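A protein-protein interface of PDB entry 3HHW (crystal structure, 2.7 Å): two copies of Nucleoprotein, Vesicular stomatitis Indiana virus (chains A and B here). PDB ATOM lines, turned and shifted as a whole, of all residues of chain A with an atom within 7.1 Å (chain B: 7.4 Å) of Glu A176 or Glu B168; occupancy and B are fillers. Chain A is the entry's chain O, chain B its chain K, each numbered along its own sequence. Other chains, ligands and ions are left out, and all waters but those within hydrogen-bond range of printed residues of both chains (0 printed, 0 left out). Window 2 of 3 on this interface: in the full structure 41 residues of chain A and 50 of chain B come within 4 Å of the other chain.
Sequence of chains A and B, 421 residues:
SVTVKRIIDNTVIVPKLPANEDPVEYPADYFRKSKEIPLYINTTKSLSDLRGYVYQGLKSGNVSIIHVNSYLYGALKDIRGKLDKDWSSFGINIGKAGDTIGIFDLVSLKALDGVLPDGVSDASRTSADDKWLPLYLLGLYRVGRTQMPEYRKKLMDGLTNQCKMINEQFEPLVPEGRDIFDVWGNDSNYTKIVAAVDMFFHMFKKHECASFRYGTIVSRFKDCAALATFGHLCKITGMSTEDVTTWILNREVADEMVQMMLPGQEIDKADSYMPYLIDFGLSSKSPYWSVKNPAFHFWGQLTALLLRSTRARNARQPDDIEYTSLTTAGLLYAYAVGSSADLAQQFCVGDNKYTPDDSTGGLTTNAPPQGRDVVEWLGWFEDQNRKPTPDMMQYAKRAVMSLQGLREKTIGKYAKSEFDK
The backbone carbonyl oxygen of Asp A179 sits close to the side-chain carboxylate of Glu B168 (3.0 Å).
The side-chain hydroxyl (OG1) of Thr B160 lies within hydrogen-bond range of the backbone carbonyl oxygen (O) of Met B156 (3.0 Å).
O of Leu B159 lies within hydrogen-bond range of SG of Cys B163 (3.3 Å).
OE2 of Glu B168 sits close to SG of Cys B163, 3.8 Å away.
Among the printed residues, merely in contact across the chains: Asp A179 with Met B156, Ile A180 with Glu B168, Glu A176 with Glu B168, Val A183 with Cys B163, Val A183 with Lys B164 and Glu A176 with Phe B170.
Glu A176 touches just these residues of chain B: Glu B168 and Phe B170.
Of the printed residues of chain B, Val A183 touches Cys B163 (3.7 Å) and Lys B164 (3.7 Å).
Of the printed residues of chain A, Met B156 touches Asp A179.
Of the printed residues of chain A, Cys B163 touches Val A183 (3.7 Å).
Printed residues of chain A within 4 Å of Lys B164: Val A183.
Glu B168 touches three residues of chain A.
Printed residues of chain A within 4 Å of Phe B170: Glu A176 (3.9 Å).
The nearest residue of chain B that does not touch Glu A176 is Cys B163 (6.4 Å).
Of the 12 printed residues of chain B, 5 touch a printed residue of chain A.
Printed residues of chain B that touch a printed residue of chain A: Met B156, Cys B163, Lys B164, Glu B168 and Phe B170.
Hydrophobic or aromatic side chains of chain B within 4 Å of the printed part of chain A: Met B156 and Phe B170.
Hydrophobic or aromatic side chains of chain A that line the printed part of chain B: Ile A180 and Val A183.
No position is printed for both chains.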
ATOM      1  N   GLY A  61     -32.643  12.559  26.620  1.00  0.00           N
ATOM      2  CA  GLY A  61     -31.227  12.481  26.257  1.00  0.00           C
ATOM      3  C   GLY A  61     -30.384  11.557  27.119  1.00  0.00           C
ATOM      4  O   GLY A  61     -30.865  11.006  28.113  1.00  0.00           O
ATOM      5  N   ASN A  62     -29.115  11.411  26.729  1.00  0.00           N
ATOM      6  CA  ASN A  62     -28.129  10.529  27.386  1.00  0.00           C
ATOM      7  C   ASN A  62     -28.640   9.154  27.847  1.00  0.00           C
ATOM      8  O   ASN A  62     -28.941   8.940  29.025  1.00  0.00           O
ATOM      9  CB  ASN A  62     -27.337  11.259  28.492  1.00  0.00           C
ATOM     10  CG  ASN A  62     -28.225  12.056  29.438  1.00  0.00           C
ATOM     11  OD1 ASN A  62     -28.968  11.492  30.243  1.00  0.00           O
ATOM     12  ND2 ASN A  62     -28.135  13.379  29.354  1.00  0.00           N
ATOM     13  N   VAL A  63     -28.725   8.233  26.892  1.00  0.00           N
ATOM     14  CA  VAL A  63     -29.177   6.867  27.146  1.00  0.00           C
ATOM     15  C   VAL A  63     -27.977   5.924  27.305  1.00  0.00           C
ATOM     16  O   VAL A  63     -26.880   6.219  26.824  1.00  0.00           O
ATOM     17  CB  VAL A  63     -30.148   6.377  26.023  1.00  0.00           C
ATOM     18  CG1 VAL A  63     -29.415   6.171  24.695  1.00  0.00           C
ATOM     19  CG2 VAL A  63     -30.897   5.113  26.444  1.00  0.00           C
ATOM     20  N   PRO A 172     -36.825  12.007  20.785  1.00  0.00           N
ATOM     21  CA  PRO A 172     -35.685  12.933  20.837  1.00  0.00           C
ATOM     22  C   PRO A 172     -36.084  14.397  20.654  1.00  0.00           C
ATOM     23  O   PRO A 172     -37.134  14.685  20.072  1.00  0.00           O
ATOM     24  CB  PRO A 172     -34.796  12.475  19.668  1.00  0.00           C
ATOM     25  CG  PRO A 172     -35.459  11.249  19.088  1.00  0.00           C
ATOM     26  CD  PRO A 172     -36.890  11.323  19.484  1.00  0.00           C
ATOM     27  N   LEU A 173     -35.243  15.305  21.147  1.00  0.00           N
ATOM     28  CA  LEU A 173     -35.518  16.742  21.087  1.00  0.00           C
ATOM     29  C   LEU A 173     -34.949  17.419  19.835  1.00  0.00           C
ATOM     30  O   LEU A 173     -34.521  16.745  18.894  1.00  0.00           O
ATOM     31  CB  LEU A 173     -35.029  17.440  22.364  1.00  0.00           C
ATOM     32  CG  LEU A 173     -36.016  17.477  23.536  1.00  0.00           C
ATOM     33  CD1 LEU A 173     -35.286  17.584  24.863  1.00  0.00           C
ATOM     34  CD2 LEU A 173     -37.026  18.613  23.383  1.00  0.00           C
ATOM     35  N   VAL A 174     -34.955  18.752  19.837  1.00  0.00           N
ATOM     36  CA  VAL A 174     -34.568  19.551  18.669  1.00  0.00           C
ATOM     37  C   VAL A 174     -33.062  19.880  18.602  1.00  0.00           C
ATOM     38  O   VAL A 174     -32.424  19.582  17.589  1.00  0.00           O
ATOM     39  CB  VAL A 174     -35.430  20.851  18.538  1.00  0.00           C
ATOM     40  CG1 VAL A 174     -35.109  21.598  17.247  1.00  0.00           C
ATOM     41  CG2 VAL A 174     -36.920  20.525  18.601  1.00  0.00           C
ATOM     42  N   PRO A 175     -32.490  20.491  19.667  1.00  0.00           N
ATOM     43  CA  PRO A 175     -31.077  20.888  19.597  1.00  0.00           C
ATOM     44  C   PRO A 175     -30.095  19.712  19.649  1.00  0.00           C
ATOM     45  O   PRO A 175     -29.285  19.553  18.733  1.00  0.00           O
ATOM     46  CB  PRO A 175     -30.901  21.800  20.824  1.00  0.00           C
ATOM     47  CG  PRO A 175     -32.294  22.083  21.319  1.00  0.00           C
ATOM     48  CD  PRO A 175     -33.076  20.870  20.964  1.00  0.00           C
ATOM     49  N   GLU A 176     -30.168  18.904  20.706  1.00  0.00           N
ATOM     50  CA  GLU A 176     -29.284  17.743  20.865  1.00  0.00           C
ATOM     51  C   GLU A 176     -29.957  16.434  20.443  1.00  0.00           C
ATOM     52  O   GLU A 176     -29.747  15.384  21.059  1.00  0.00           O
ATOM     53  CB  GLU A 176     -28.763  17.646  22.303  1.00  0.00           C
ATOM     54  CG  GLU A 176     -27.614  18.595  22.621  1.00  0.00           C
ATOM     55  CD  GLU A 176     -26.907  18.253  23.921  1.00  0.00           C
ATOM     56  OE1 GLU A 176     -27.591  17.912  24.911  1.00  0.00           O
ATOM     57  OE2 GLU A 176     -25.661  18.333  23.956  1.00  0.00           O
ATOM     58  N   GLY A 177     -30.760  16.507  19.383  1.00  0.00           N
ATOM     59  CA  GLY A 177     -31.473  15.347  18.858  1.00  0.00           C
ATOM     60  C   GLY A 177     -30.579  14.376  18.109  1.00  0.00           C
ATOM     61  O   GLY A 177     -30.804  13.168  18.153  1.00  0.00           O
ATOM     62  N   ARG A 178     -29.562  14.907  17.431  1.00  0.00           N
ATOM     63  CA  ARG A 178     -28.650  14.100  16.617  1.00  0.00           C
ATOM     64  C   ARG A 178     -27.345  13.760  17.346  1.00  0.00           C
ATOM     65  O   ARG A 178     -26.559  12.934  16.874  1.00  0.00           O
ATOM     66  CB  ARG A 178     -28.339  14.825  15.303  1.00  0.00           C
ATOM     67  CG  ARG A 178     -27.992  13.902  14.137  1.00  0.00           C
ATOM     68  CD  ARG A 178     -27.057  14.570  13.132  1.00  0.00           C
ATOM     69  NE  ARG A 178     -27.643  15.756  12.506  1.00  0.00           N
ATOM     70  CZ  ARG A 178     -27.330  17.011  12.819  1.00  0.00           C
ATOM     71  NH1 ARG A 178     -26.427  17.269  13.759  1.00  0.00           N
ATOM     72  NH2 ARG A 178     -27.924  18.016  12.191  1.00  0.00           N
ATOM     73  N   ASP A 179     -27.124  14.389  18.499  1.00  0.00           N
ATOM     74  CA  ASP A 179     -25.884  14.217  19.260  1.00  0.00           C
ATOM     75  C   ASP A 179     -25.837  12.938  20.107  1.00  0.00           C
ATOM     76  O   ASP A 179     -24.887  12.725  20.865  1.00  0.00           O
ATOM     77  CB  ASP A 179     -25.624  15.450  20.134  1.00  0.00           C
ATOM     78  CG  ASP A 179     -25.271  16.683  19.318  1.00  0.00           C
ATOM     79  OD1 ASP A 179     -24.406  16.584  18.422  1.00  0.00           O
ATOM     80  OD2 ASP A 179     -25.855  17.756  19.582  1.00  0.00           O
ATOM     81  N   ILE A 180     -26.856  12.090  19.968  1.00  0.00           N
ATOM     82  CA  ILE A 180     -26.947  10.847  20.742  1.00  0.00           C
ATOM     83  C   ILE A 180     -26.987   9.570  19.888  1.00  0.00           C
ATOM     84  O   ILE A 180     -26.852   8.465  20.419  1.00  0.00           O
ATOM     85  CB  ILE A 180     -28.147  10.860  21.742  1.00  0.00           C
ATOM     86  CG1 ILE A 180     -29.453  11.251  21.034  1.00  0.00           C
ATOM     87  CG2 ILE A 180     -27.849  11.786  22.925  1.00  0.00           C
ATOM     88  CD1 ILE A 180     -30.716  10.935  21.823  1.00  0.00           C
ATOM     89  N   PHE A 181     -27.161   9.724  18.575  1.00  0.00           N
ATOM     90  CA  PHE A 181     -27.250   8.574  17.665  1.00  0.00           C
ATOM     91  C   PHE A 181     -25.910   8.194  17.029  1.00  0.00           C
ATOM     92  O   PHE A 181     -25.682   7.027  16.704  1.00  0.00           O
ATOM     93  CB  PHE A 181     -28.293   8.811  16.561  1.00  0.00           C
ATOM     94  CG  PHE A 181     -29.655   9.218  17.069  1.00  0.00           C
ATOM     95  CD1 PHE A 181     -30.237   8.581  18.163  1.00  0.00           C
ATOM     96  CD2 PHE A 181     -30.367  10.228  16.426  1.00  0.00           C
ATOM     97  CE1 PHE A 181     -31.497   8.961  18.623  1.00  0.00           C
ATOM     98  CE2 PHE A 181     -31.630  10.608  16.873  1.00  0.00           C
ATOM     99  CZ  PHE A 181     -32.194   9.976  17.976  1.00  0.00           C
ATOM    100  N   VAL A 183     -23.119   8.096  18.414  1.00  0.00           N
ATOM    101  CA  VAL A 183     -22.403   7.277  19.392  1.00  0.00           C
ATOM    102  C   VAL A 183     -22.633   5.791  19.100  1.00  0.00           C
ATOM    103  O   VAL A 183     -21.718   4.972  19.222  1.00  0.00           O
ATOM    104  CB  VAL A 183     -22.871   7.610  20.837  1.00  0.00           C
ATOM    105  CG1 VAL A 183     -22.259   6.655  21.860  1.00  0.00           C
ATOM    106  CG2 VAL A 183     -22.546   9.057  21.188  1.00  0.00           C
ATOM    107  N   TRP B 132     -12.482  10.477  28.790  1.00  0.00           N
ATOM    108  CA  TRP B 132     -12.562  11.551  27.786  1.00  0.00           C
ATOM    109  C   TRP B 132     -11.586  12.727  27.914  1.00  0.00           C
ATOM    110  O   TRP B 132     -11.264  13.369  26.912  1.00  0.00           O
ATOM    111  CB  TRP B 132     -13.999  12.079  27.669  1.00  0.00           C
ATOM    112  CG  TRP B 132     -14.542  12.717  28.919  1.00  0.00           C
ATOM    113  CD1 TRP B 132     -15.274  12.107  29.893  1.00  0.00           C
ATOM    114  CD2 TRP B 132     -14.412  14.092  29.317  1.00  0.00           C
ATOM    115  NE1 TRP B 132     -15.605  13.008  30.877  1.00  0.00           N
ATOM    116  CE2 TRP B 132     -15.088  14.233  30.550  1.00  0.00           C
ATOM    117  CE3 TRP B 132     -13.789  15.214  28.756  1.00  0.00           C
ATOM    118  CZ2 TRP B 132     -15.158  15.453  31.232  1.00  0.00           C
ATOM    119  CZ3 TRP B 132     -13.860  16.428  29.435  1.00  0.00           C
ATOM    120  CH2 TRP B 132     -14.541  16.535  30.660  1.00  0.00           C
ATOM    121  N   MET B 156     -15.920  20.213  18.147  1.00  0.00           N
ATOM    122  CA  MET B 156     -17.152  19.411  18.144  1.00  0.00           C
ATOM    123  C   MET B 156     -16.881  17.954  17.748  1.00  0.00           C
ATOM    124  O   MET B 156     -17.500  17.032  18.290  1.00  0.00           O
ATOM    125  CB  MET B 156     -18.188  20.034  17.196  1.00  0.00           C
ATOM    126  CG  MET B 156     -19.544  19.327  17.128  1.00  0.00           C
ATOM    127  SD  MET B 156     -20.622  19.649  18.540  1.00  0.00           S
ATOM    128  CE  MET B 156     -22.175  18.997  17.935  1.00  0.00           C
ATOM    129  N   LEU B 159     -15.239  16.268  20.674  1.00  0.00           N
ATOM    130  CA  LEU B 159     -16.205  16.118  21.765  1.00  0.00           C
ATOM    131  C   LEU B 159     -17.257  15.040  21.473  1.00  0.00           C
ATOM    132  O   LEU B 159     -18.167  14.821  22.275  1.00  0.00           O
ATOM    133  CB  LEU B 159     -16.877  17.461  22.090  1.00  0.00           C
ATOM    134  CG  LEU B 159     -16.064  18.534  22.832  1.00  0.00           C
ATOM    135  CD1 LEU B 159     -16.665  19.913  22.605  1.00  0.00           C
ATOM    136  CD2 LEU B 159     -15.945  18.239  24.324  1.00  0.00           C
ATOM    137  N   THR B 160     -17.123  14.374  20.326  1.00  0.00           N
ATOM    138  CA  THR B 160     -17.994  13.254  19.963  1.00  0.00           C
ATOM    139  C   THR B 160     -17.656  12.022  20.810  1.00  0.00           C
ATOM    140  O   THR B 160     -18.552  11.278  21.214  1.00  0.00           O
ATOM    141  CB  THR B 160     -17.894  12.900  18.456  1.00  0.00           C
ATOM    142  OG1 THR B 160     -17.701  14.093  17.686  1.00  0.00           O
ATOM    143  CG2 THR B 160     -19.160  12.199  17.979  1.00  0.00           C
ATOM    144  N   GLN B 162     -16.416  12.201  23.762  1.00  0.00           N
ATOM    145  CA  GLN B 162     -16.839  12.578  25.110  1.00  0.00           C
ATOM    146  C   GLN B 162     -18.241  12.044  25.389  1.00  0.00           C
ATOM    147  O   GLN B 162     -18.583  11.740  26.534  1.00  0.00           O
ATOM    148  CB  GLN B 162     -16.819  14.104  25.264  1.00  0.00           C
ATOM    149  CG  GLN B 162     -15.473  14.707  25.681  1.00  0.00           C
ATOM    150  CD  GLN B 162     -14.361  14.545  24.645  1.00  0.00           C
ATOM    151  OE1 GLN B 162     -13.993  13.431  24.268  1.00  0.00           O
ATOM    152  NE2 GLN B 162     -13.802  15.667  24.205  1.00  0.00           N
ATOM    153  N   CYS B 163     -19.037  11.938  24.327  1.00  0.00           N
ATOM    154  CA  CYS B 163     -20.382  11.372  24.389  1.00  0.00           C
ATOM    155  C   CYS B 163     -20.351   9.850  24.242  1.00  0.00           C
ATOM    156  O   CYS B 163     -21.296   9.161  24.633  1.00  0.00           O
ATOM    157  CB  CYS B 163     -21.262  11.975  23.288  1.00  0.00           C
ATOM    158  SG  CYS B 163     -21.175  13.777  23.124  1.00  0.00           S
ATOM    159  N   LYS B 164     -19.259   9.337  23.676  1.00  0.00           N
ATOM    160  CA  LYS B 164     -19.113   7.907  23.391  1.00  0.00           C
ATOM    161  C   LYS B 164     -18.592   7.094  24.576  1.00  0.00           C
ATOM    162  O   LYS B 164     -18.655   5.862  24.559  1.00  0.00           O
ATOM    163  CB  LYS B 164     -18.212   7.693  22.168  1.00  0.00           C
ATOM    164  CG  LYS B 164     -18.873   8.027  20.840  1.00  0.00           C
ATOM    165  CD  LYS B 164     -17.858   8.086  19.712  1.00  0.00           C
ATOM    166  CE  LYS B 164     -18.502   8.563  18.421  1.00  0.00           C
ATOM    167  NZ  LYS B 164     -17.512   8.682  17.316  1.00  0.00           N
ATOM    168  N   ILE B 166     -18.686   8.541  28.345  1.00  0.00           N
ATOM    169  CA  ILE B 166     -19.561   8.859  29.486  1.00  0.00           C
ATOM    170  C   ILE B 166     -20.455  10.082  29.166  1.00  0.00           C
ATOM    171  O   ILE B 166     -20.793  10.302  27.998  1.00  0.00           O
ATOM    172  CB  ILE B 166     -18.752   8.974  30.834  1.00  0.00           C
ATOM    173  CG1 ILE B 166     -19.655   8.706  32.048  1.00  0.00           C
ATOM    174  CG2 ILE B 166     -17.978  10.298  30.930  1.00  0.00           C
ATOM    175  CD1 ILE B 166     -18.908   8.319  33.315  1.00  0.00           C
ATOM    176  N   ASN B 167     -20.842  10.851  30.185  1.00  0.00           N
ATOM    177  CA  ASN B 167     -21.708  12.024  30.018  1.00  0.00           C
ATOM    178  C   ASN B 167     -21.177  13.059  29.024  1.00  0.00           C
ATOM    179  O   ASN B 167     -19.964  13.251  28.900  1.00  0.00           O
ATOM    180  CB  ASN B 167     -21.976  12.691  31.373  1.00  0.00           C
ATOM    181  CG  ASN B 167     -22.832  11.833  32.293  1.00  0.00           C
ATOM    182  OD1 ASN B 167     -22.591  10.635  32.455  1.00  0.00           O
ATOM    183  ND2 ASN B 167     -23.832  12.450  32.911  1.00  0.00           N
ATOM    184  N   GLU B 168     -22.098  13.717  28.323  1.00  0.00           N
ATOM    185  CA  GLU B 168     -21.757  14.709  27.302  1.00  0.00           C
ATOM    186  C   GLU B 168     -21.404  16.048  27.949  1.00  0.00           C
ATOM    187  O   GLU B 168     -22.277  16.734  28.489  1.00  0.00           O
ATOM    188  CB  GLU B 168     -22.913  14.888  26.308  1.00  0.00           C
ATOM    189  CG  GLU B 168     -23.551  13.582  25.823  1.00  0.00           C
ATOM    190  CD  GLU B 168     -24.512  13.775  24.657  1.00  0.00           C
ATOM    191  OE1 GLU B 168     -25.065  14.885  24.499  1.00  0.00           O
ATOM    192  OE2 GLU B 168     -24.718  12.805  23.897  1.00  0.00           O
ATOM    193  N   GLN B 169     -20.123  16.411  27.898  1.00  0.00           N
ATOM    194  CA  GLN B 169     -19.646  17.654  28.510  1.00  0.00           C
ATOM    195  C   GLN B 169     -18.656  18.424  27.641  1.00  0.00           C
ATOM    196  O   GLN B 169     -17.810  17.833  26.964  1.00  0.00           O
ATOM    197  CB  GLN B 169     -19.034  17.387  29.890  1.00  0.00           C
ATOM    198  CG  GLN B 169     -20.057  17.237  31.012  1.00  0.00           C
ATOM    199  CD  GLN B 169     -19.447  17.378  32.395  1.00  0.00           C
ATOM    200  OE1 GLN B 169     -18.489  18.126  32.596  1.00  0.00           O
ATOM    201  NE2 GLN B 169     -20.008  16.662  33.363  1.00  0.00           N
ATOM    202  N   PHE B 170     -18.777  19.749  27.680  1.00  0.00           N
ATOM    203  CA  PHE B 170     -17.884  20.659  26.963  1.00  0.00           C
ATOM    204  C   PHE B 170     -17.041  21.441  27.972  1.00  0.00           C
ATOM    205  O   PHE B 170     -17.440  21.593  29.132  1.00  0.00           O
ATOM    206  CB  PHE B 170     -18.686  21.640  26.094  1.00  0.00           C
ATOM    207  CG  PHE B 170     -19.890  21.030  25.420  1.00  0.00           C
ATOM    208  CD1 PHE B 170     -21.163  21.191  25.963  1.00  0.00           C
ATOM    209  CD2 PHE B 170     -19.754  20.305  24.238  1.00  0.00           C
ATOM    210  CE1 PHE B 170     -22.281  20.633  25.344  1.00  0.00           C
ATOM    211  CE2 PHE B 170     -20.865  19.743  23.611  1.00  0.00           C
ATOM    212  CZ  PHE B 170     -22.130  19.908  24.166  1.00  0.00           C
